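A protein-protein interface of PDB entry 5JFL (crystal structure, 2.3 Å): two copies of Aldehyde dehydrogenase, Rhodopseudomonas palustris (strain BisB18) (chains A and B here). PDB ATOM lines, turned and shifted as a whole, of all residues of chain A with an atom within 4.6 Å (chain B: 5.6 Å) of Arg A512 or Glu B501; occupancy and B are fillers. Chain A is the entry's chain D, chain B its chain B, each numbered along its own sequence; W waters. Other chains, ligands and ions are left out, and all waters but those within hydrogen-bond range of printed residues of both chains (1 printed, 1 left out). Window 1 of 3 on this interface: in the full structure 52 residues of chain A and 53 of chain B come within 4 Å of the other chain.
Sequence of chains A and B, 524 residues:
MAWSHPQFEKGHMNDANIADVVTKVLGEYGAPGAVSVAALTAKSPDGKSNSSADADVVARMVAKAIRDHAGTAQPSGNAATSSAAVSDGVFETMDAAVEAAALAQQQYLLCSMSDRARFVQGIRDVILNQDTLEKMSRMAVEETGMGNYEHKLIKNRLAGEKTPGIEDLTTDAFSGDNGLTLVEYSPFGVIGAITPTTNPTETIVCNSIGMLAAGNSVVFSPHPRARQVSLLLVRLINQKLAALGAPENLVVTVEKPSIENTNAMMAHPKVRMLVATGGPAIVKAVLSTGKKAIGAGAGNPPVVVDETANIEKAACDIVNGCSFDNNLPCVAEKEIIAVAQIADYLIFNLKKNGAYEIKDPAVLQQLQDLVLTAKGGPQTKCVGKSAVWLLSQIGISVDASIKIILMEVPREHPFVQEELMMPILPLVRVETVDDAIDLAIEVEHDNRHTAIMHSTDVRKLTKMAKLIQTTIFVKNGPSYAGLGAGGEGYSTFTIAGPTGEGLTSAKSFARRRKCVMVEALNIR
The backbone carbonyl oxygen (O) of Thr B471 is in hydrogen-bond range of the backbone NH (N) of Lys A514 (2.5 Å). O of Gly B500 sits at hydrogen-bond distance from N of Arg A512 (3.1 Å). The side-chain amino group of Lys A292 lies close to the side-chain amino group of Lys B292, 3.2 Å away. The side-chain carboxylate (OE2) of Glu B501 lies within salt-bridge range of the side-chain amino group (NZ) of Lys A292, 3.3 Å away.
The backbone NH (N) of Gly B295 sits close to the side-chain hydroxyl (OG1) of Thr B499 (3.5 Å). N of Ala B496 lies within hydrogen-bond range of O of Gly B502 (2.9 Å). The backbone NH (N) of Arg A513 sits at hydrogen-bond distance from the backbone carbonyl oxygen (O) of Glu A184 (2.8 Å). OH of Tyr A185 sits at hydrogen-bond distance from NH2 of Arg A512, at 2.8 Å. The side-chain hydroxyl (OG1) of Thr B499 is in hydrogen-bond range of the side-chain carboxylate (OE1) of Glu B501 (2.6 Å). The side-chain carboxylate of Asp A172 lies within salt-bridge range of the guanidinium group of Arg A512.
CE of Lys A292 touches O of Thr B499, 3.3 Å away. NH2 of Arg A511 touches CG2 of Thr B471, 3.3 Å away. CA of Arg A511 touches O of Gly B500 (3.7 Å). Thr B471 touches Arg A512 (CB to O, 3.9 Å). Arg A512 touches Glu B501. Arg A512 touches Gly B502 (O to CA, 3.8 Å). Thr B471 touches Arg A513 (O to C, 3.5 Å). NZ of Lys A514 touches CD2 of Leu B503, 3.4 Å away.
Val A183 touches none of the printed residues of chain B. Tyr A185 touches none of the printed residues of chain B. Of chain B, only Thr B471 (3.9 Å), Gly B500 (3.1 Å), Glu B501 (3.9 Å) and Gly B502 (3.8 Å) come within 4 Å of Arg A512. Printed residues of chain B within 4 Å of Lys A514: Thr B471 (2.5 Å) and Leu B503 (3.4 Å). Of the printed residues of chain A, Lys B292 touches Lys A292 (3.2 Å). Printed residues of chain A within 4 Å of Thr B499: Lys A292. Of chain A, only Lys A292 (3.3 Å) and Arg A512 (3.9 Å) come within 4 Å of Glu B501. Of the printed residues of chain A, Leu B503 touches Lys A514. The nearest residue of chain B that does not touch Arg A512 is Lys B507 (5.0 Å). The nearest printed residue of chain A that does not touch Glu B501 is Arg A511 (5.8 Å). The nearest printed residue of chain A that does not touch Lys B292 is Ala A510 (10.1 Å).
Of the 10 printed residues of chain A, 5 touch a printed residue of chain B. Printed residues of chain A that touch a printed residue of chain B: Lys A292, Arg A511, Arg A512, Arg A513 and Lys A514. Of the 14 printed residues of chain B, 7 touch a printed residue of chain A. Among the printed residues, Asp or Glu carboxylates within 4 Å of a Lys or Arg side-chain nitrogen of the other chain: Lys A292 with Glu B501.
Lys B292 touches its own counterpart, Lys A292. 1 position is printed for both chains. Of the 12 pairs that touch across the chains among the printed residues, 1 has its exchanged pair printed and touching as well.
Water W1 lies within hydrogen-bond range of the side-chain amino group of Lys B292 (2.8 Å), the side-chain amino group of Lys A292 (2.8 Å), the backbone carbonyl oxygen of Ala B293 (2.9 Å) and the side-chain carboxylate of Glu B501 (3.3 Å).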
ATOM      1  N   ASP A 172       4.591  14.191  15.491  1.00  0.00           N
ATOM      2  CA  ASP A 172       3.282  13.654  15.828  1.00  0.00           C
ATOM      3  C   ASP A 172       2.749  14.362  17.067  1.00  0.00           C
ATOM      4  O   ASP A 172       3.513  14.752  17.953  1.00  0.00           O
ATOM      5  CB  ASP A 172       3.359  12.147  16.071  1.00  0.00           C
ATOM      6  CG  ASP A 172       3.579  11.367  14.792  1.00  0.00           C
ATOM      7  OD1 ASP A 172       2.931  11.701  13.780  1.00  0.00           O
ATOM      8  OD2 ASP A 172       4.416  10.439  14.792  1.00  0.00           O
ATOM      9  N   VAL A 183       5.644  13.622  19.809  1.00  0.00           N
ATOM     10  CA  VAL A 183       6.711  12.659  19.565  1.00  0.00           C
ATOM     11  C   VAL A 183       7.610  13.204  18.465  1.00  0.00           C
ATOM     12  O   VAL A 183       7.135  13.594  17.391  1.00  0.00           O
ATOM     13  CB  VAL A 183       6.176  11.257  19.216  1.00  0.00           C
ATOM     14  CG1 VAL A 183       7.316  10.238  19.278  1.00  0.00           C
ATOM     15  CG2 VAL A 183       5.069  10.845  20.180  1.00  0.00           C
ATOM     16  N   GLU A 184       8.912  13.198  18.744  1.00  0.00           N
ATOM     17  CA  GLU A 184       9.912  13.910  17.974  1.00  0.00           C
ATOM     18  C   GLU A 184      11.047  12.990  17.584  1.00  0.00           C
ATOM     19  O   GLU A 184      11.418  12.099  18.344  1.00  0.00           O
ATOM     20  CB  GLU A 184      10.518  15.037  18.774  1.00  0.00           C
ATOM     21  CG  GLU A 184      10.020  16.423  18.427  1.00  0.00           C
ATOM     22  CD  GLU A 184      10.162  16.765  16.981  1.00  0.00           C
ATOM     23  OE1 GLU A 184       9.522  17.731  16.546  1.00  0.00           O
ATOM     24  OE2 GLU A 184      10.920  16.088  16.245  1.00  0.00           O
ATOM     25  N   TYR A 185      11.669  13.288  16.448  1.00  0.00           N
ATOM     26  CA  TYR A 185      12.905  12.628  16.056  1.00  0.00           C
ATOM     27  C   TYR A 185      14.087  13.451  16.555  1.00  0.00           C
ATOM     28  O   TYR A 185      14.278  14.588  16.118  1.00  0.00           O
ATOM     29  CB  TYR A 185      12.985  12.467  14.540  1.00  0.00           C
ATOM     30  CG  TYR A 185      11.970  11.527  13.940  1.00  0.00           C
ATOM     31  CD1 TYR A 185      12.206  10.160  13.897  1.00  0.00           C
ATOM     32  CD2 TYR A 185      10.783  12.007  13.402  1.00  0.00           C
ATOM     33  CE1 TYR A 185      11.288   9.296  13.342  1.00  0.00           C
ATOM     34  CE2 TYR A 185       9.855  11.147  12.844  1.00  0.00           C
ATOM     35  CZ  TYR A 185      10.113   9.792  12.818  1.00  0.00           C
ATOM     36  OH  TYR A 185       9.196   8.929  12.264  1.00  0.00           O
ATOM     37  N   LYS A 292      23.477  -0.014  18.326  1.00  0.00           N
ATOM     38  CA  LYS A 292      22.439   0.110  17.313  1.00  0.00           C
ATOM     39  C   LYS A 292      23.085   0.213  15.936  1.00  0.00           C
ATOM     40  O   LYS A 292      24.054   0.954  15.748  1.00  0.00           O
ATOM     41  CB  LYS A 292      21.576   1.340  17.602  1.00  0.00           C
ATOM     42  CG  LYS A 292      20.710   1.817  16.444  1.00  0.00           C
ATOM     43  CD  LYS A 292      19.514   0.915  16.205  1.00  0.00           C
ATOM     44  CE  LYS A 292      18.537   1.561  15.234  1.00  0.00           C
ATOM     45  NZ  LYS A 292      17.414   0.654  14.875  1.00  0.00           N
ATOM     46  N   ALA A 510      17.678   9.094  13.630  1.00  0.00           N
ATOM     47  CA  ALA A 510      17.268   9.877  14.784  1.00  0.00           C
ATOM     48  C   ALA A 510      16.551   8.988  15.792  1.00  0.00           C
ATOM     49  O   ALA A 510      16.050   7.911  15.459  1.00  0.00           O
ATOM     50  CB  ALA A 510      16.362  11.046  14.370  1.00  0.00           C
ATOM     51  N   ARG A 511      16.518   9.454  17.039  1.00  0.00           N
ATOM     52  CA  ARG A 511      15.820   8.775  18.122  1.00  0.00           C
ATOM     53  C   ARG A 511      14.455   9.410  18.340  1.00  0.00           C
ATOM     54  O   ARG A 511      14.304  10.632  18.251  1.00  0.00           O
ATOM     55  CB  ARG A 511      16.611   8.837  19.429  1.00  0.00           C
ATOM     56  CG  ARG A 511      18.106   8.710  19.277  1.00  0.00           C
ATOM     57  CD  ARG A 511      18.832   9.141  20.544  1.00  0.00           C
ATOM     58  NE  ARG A 511      18.232   8.600  21.757  1.00  0.00           N
ATOM     59  CZ  ARG A 511      17.593   9.333  22.663  1.00  0.00           C
ATOM     60  NH1 ARG A 511      17.468  10.642  22.491  1.00  0.00           N
ATOM     61  NH2 ARG A 511      17.082   8.758  23.740  1.00  0.00           N
ATOM     62  N   ARG A 512      13.467   8.575  18.646  1.00  0.00           N
ATOM     63  CA  ARG A 512      12.122   9.058  18.917  1.00  0.00           C
ATOM     64  C   ARG A 512      11.966   9.378  20.398  1.00  0.00           C
ATOM     65  O   ARG A 512      12.271   8.545  21.256  1.00  0.00           O
ATOM     66  CB  ARG A 512      11.077   8.034  18.483  1.00  0.00           C
ATOM     67  CG  ARG A 512      10.390   8.406  17.189  1.00  0.00           C
ATOM     68  CD  ARG A 512       8.973   7.878  17.154  1.00  0.00           C
ATOM     69  NE  ARG A 512       8.145   8.658  16.241  1.00  0.00           N
ATOM     70  CZ  ARG A 512       7.922   8.327  14.977  1.00  0.00           C
ATOM     71  NH1 ARG A 512       8.463   7.226  14.474  1.00  0.00           N
ATOM     72  NH2 ARG A 512       7.157   9.097  14.215  1.00  0.00           N
ATOM     73  N   ARG A 513      11.484  10.583  20.686  1.00  0.00           N
ATOM     74  CA  ARG A 513      11.258  11.042  22.047  1.00  0.00           C
ATOM     75  C   ARG A 513       9.802  11.444  22.218  1.00  0.00           C
ATOM     76  O   ARG A 513       9.194  12.011  21.307  1.00  0.00           O
ATOM     77  CB  ARG A 513      12.170  12.218  22.390  1.00  0.00           C
ATOM     78  CG  ARG A 513      13.633  11.845  22.460  1.00  0.00           C
ATOM     79  CD  ARG A 513      14.492  13.031  22.841  1.00  0.00           C
ATOM     80  NE  ARG A 513      14.012  13.710  24.040  1.00  0.00           N
ATOM     81  CZ  ARG A 513      13.566  14.962  24.062  1.00  0.00           C
ATOM     82  NH1 ARG A 513      13.542  15.680  22.946  1.00  0.00           N
ATOM     83  NH2 ARG A 513      13.151  15.499  25.202  1.00  0.00           N
ATOM     84  N   LYS A 514       9.253  11.153  23.392  1.00  0.00           N
ATOM     85  CA  LYS A 514       7.858  11.429  23.713  1.00  0.00           C
ATOM     86  C   LYS A 514       7.816  12.483  24.808  1.00  0.00           C
ATOM     87  O   LYS A 514       8.393  12.286  25.884  1.00  0.00           O
ATOM     88  CB  LYS A 514       7.148  10.150  24.160  1.00  0.00           C
ATOM     89  CG  LYS A 514       5.675  10.311  24.469  1.00  0.00           C
ATOM     90  CD  LYS A 514       5.170   9.127  25.274  1.00  0.00           C
ATOM     91  CE  LYS A 514       3.653   9.101  25.355  1.00  0.00           C
ATOM     92  NZ  LYS A 514       3.161   7.962  26.181  1.00  0.00           N
ATOM     93  N   LYS B 292      19.334  -8.191  14.012  1.00  0.00           N
ATOM     94  CA  LYS B 292      18.507  -7.056  14.393  1.00  0.00           C
ATOM     95  C   LYS B 292      17.970  -7.258  15.803  1.00  0.00           C
ATOM     96  O   LYS B 292      17.502  -8.343  16.149  1.00  0.00           O
ATOM     97  CB  LYS B 292      17.353  -6.904  13.400  1.00  0.00           C
ATOM     98  CG  LYS B 292      16.324  -5.859  13.776  1.00  0.00           C
ATOM     99  CD  LYS B 292      16.870  -4.461  13.586  1.00  0.00           C
ATOM    100  CE  LYS B 292      15.818  -3.421  13.922  1.00  0.00           C
ATOM    101  NZ  LYS B 292      16.307  -2.040  13.652  1.00  0.00           N
ATOM    102  N   ALA B 293      18.059  -6.216  16.624  1.00  0.00           N
ATOM    103  CA  ALA B 293      17.644  -6.335  18.013  1.00  0.00           C
ATOM    104  C   ALA B 293      17.094  -5.007  18.509  1.00  0.00           C
ATOM    105  O   ALA B 293      17.595  -3.941  18.140  1.00  0.00           O
ATOM    106  CB  ALA B 293      18.803  -6.789  18.906  1.00  0.00           C
ATOM    107  N   ILE B 294      16.061  -5.084  19.343  1.00  0.00           N
ATOM    108  CA  ILE B 294      15.505  -3.925  20.032  1.00  0.00           C
ATOM    109  C   ILE B 294      15.868  -4.045  21.506  1.00  0.00           C
ATOM    110  O   ILE B 294      15.499  -5.021  22.169  1.00  0.00           O
ATOM    111  CB  ILE B 294      13.985  -3.816  19.836  1.00  0.00           C
ATOM    112  CG1 ILE B 294      13.669  -3.299  18.430  1.00  0.00           C
ATOM    113  CG2 ILE B 294      13.372  -2.910  20.896  1.00  0.00           C
ATOM    114  CD1 ILE B 294      12.209  -2.960  18.216  1.00  0.00           C
ATOM    115  N   GLY B 295      16.603  -3.059  22.015  1.00  0.00           N
ATOM    116  CA  GLY B 295      17.054  -3.081  23.392  1.00  0.00           C
ATOM    117  C   GLY B 295      16.465  -1.967  24.231  1.00  0.00           C
ATOM    118  O   GLY B 295      16.752  -0.788  24.005  1.00  0.00           O
ATOM    119  N   THR B 471      13.645   9.680  26.264  1.00  0.00           N
ATOM    120  CA  THR B 471      12.609   9.219  25.344  1.00  0.00           C
ATOM    121  C   THR B 471      11.206   9.451  25.891  1.00  0.00           C
ATOM    122  O   THR B 471      10.260   9.577  25.109  1.00  0.00           O
ATOM    123  CB  THR B 471      12.794   7.743  24.998  1.00  0.00           C
ATOM    124  OG1 THR B 471      12.231   6.931  26.033  1.00  0.00           O
ATOM    125  CG2 THR B 471      14.260   7.407  24.819  1.00  0.00           C
ATOM    126  N   ALA B 496      12.463   1.713  24.154  1.00  0.00           N
ATOM    127  CA  ALA B 496      13.782   1.630  23.536  1.00  0.00           C
ATOM    128  C   ALA B 496      14.495   2.971  23.666  1.00  0.00           C
ATOM    129  O   ALA B 496      14.130   3.947  23.002  1.00  0.00           O
ATOM    130  CB  ALA B 496      13.653   1.216  22.073  1.00  0.00           C
ATOM    131  N   THR B 499      18.439   1.864  21.312  1.00  0.00           N
ATOM    132  CA  THR B 499      18.138   1.562  19.917  1.00  0.00           C
ATOM    133  C   THR B 499      17.248   2.611  19.261  1.00  0.00           C
ATOM    134  O   THR B 499      17.139   2.620  18.030  1.00  0.00           O
ATOM    135  CB  THR B 499      17.492   0.178  19.804  1.00  0.00           C
ATOM    136  OG1 THR B 499      16.348   0.107  20.663  1.00  0.00           O
ATOM    137  CG2 THR B 499      18.488  -0.905  20.195  1.00  0.00           C
ATOM    138  N   GLY B 500      16.603   3.474  20.041  1.00  0.00           N
ATOM    139  CA  GLY B 500      15.976   4.666  19.511  1.00  0.00           C
ATOM    140  C   GLY B 500      14.565   4.524  18.980  1.00  0.00           C
ATOM    141  O   GLY B 500      14.007   5.521  18.503  1.00  0.00           O
ATOM    142  N   GLU B 501      13.964   3.334  19.036  1.00  0.00           N
ATOM    143  CA  GLU B 501      12.585   3.202  18.574  1.00  0.00           C
ATOM    144  C   GLU B 501      11.599   3.933  19.475  1.00  0.00           C
ATOM    145  O   GLU B 501      10.463   4.183  19.058  1.00  0.00           O
ATOM    146  CB  GLU B 501      12.178   1.730  18.469  1.00  0.00           C
ATOM    147  CG  GLU B 501      12.837   0.959  17.346  1.00  0.00           C
ATOM    148  CD  GLU B 501      14.131   0.298  17.790  1.00  0.00           C
ATOM    149  OE1 GLU B 501      14.314   0.107  19.002  1.00  0.00           O
ATOM    150  OE2 GLU B 501      14.953  -0.026  16.925  1.00  0.00           O
ATOM    151  N   GLY B 502      12.000   4.271  20.697  1.00  0.00           N
ATOM    152  CA  GLY B 502      11.070   4.907  21.609  1.00  0.00           C
ATOM    153  C   GLY B 502      10.065   3.903  22.139  1.00  0.00           C
ATOM    154  O   GLY B 502      10.402   2.762  22.477  1.00  0.00           O
ATOM    155  N   LEU B 503       8.807   4.327  22.206  1.00  0.00           N
ATOM    156  CA  LEU B 503       7.731   3.488  22.728  1.00  0.00           C
ATOM    157  C   LEU B 503       7.366   2.466  21.660  1.00  0.00           C
ATOM    158  O   LEU B 503       6.531   2.713  20.787  1.00  0.00           O
ATOM    159  CB  LEU B 503       6.532   4.337  23.129  1.00  0.00           C
ATOM    160  CG  LEU B 503       6.610   5.068  24.474  1.00  0.00           C
ATOM    161  CD1 LEU B 503       7.650   6.184  24.480  1.00  0.00           C
ATOM    162  CD2 LEU B 503       5.240   5.600  24.854  1.00  0.00           C
ATOM    163  N   THR B 504       8.007   1.300  21.734  1.00  0.00           N
ATOM    164  CA  THR B 504       7.785   0.258  20.742  1.00  0.00           C
ATOM    165  C   THR B 504       6.312  -0.117  20.681  1.00  0.00           C
ATOM    166  O   THR B 504       5.663  -0.316  21.711  1.00  0.00           O
ATOM    167  CB  THR B 504       8.624  -0.981  21.060  1.00  0.00           C
ATOM    168  OG1 THR B 504       8.070  -1.660  22.192  1.00  0.00           O
ATOM    169  CG2 THR B 504      10.065  -0.591  21.359  1.00  0.00           C
ATOM    170  N   LYS B 507       4.284  -1.228  14.983  1.00  0.00           N
ATOM    171  CA  LYS B 507       5.131  -0.702  13.916  1.00  0.00           C
ATOM    172  C   LYS B 507       6.608  -0.990  14.167  1.00  0.00           C
ATOM    173  O   LYS B 507       7.377  -1.162  13.214  1.00  0.00           O
ATOM    174  CB  LYS B 507       4.894   0.802  13.779  1.00  0.00           C
ATOM    175  CG  LYS B 507       5.874   1.540  12.890  1.00  0.00           C
ATOM    176  CD  LYS B 507       5.970   3.004  13.287  1.00  0.00           C
ATOM    177  CE  LYS B 507       4.593   3.646  13.388  1.00  0.00           C
ATOM    178  NZ  LYS B 507       3.889   3.680  12.078  1.00  0.00           N
ATOM    179  N   SER B 508       7.020  -1.054  15.434  1.00  0.00           N
ATOM    180  CA  SER B 508       8.426  -1.292  15.744  1.00  0.00           C
ATOM    181  C   SER B 508       8.880  -2.675  15.298  1.00  0.00           C
ATOM    182  O   SER B 508      10.061  -2.869  14.990  1.00  0.00           O
ATOM    183  CB  SER B 508       8.666  -1.117  17.243  1.00  0.00           C
ATOM    184  OG  SER B 508       8.368   0.206  17.647  1.00  0.00           O
HETATM  185  O   HOH W   1      17.552  -1.848  16.123  1.00  0.00           O
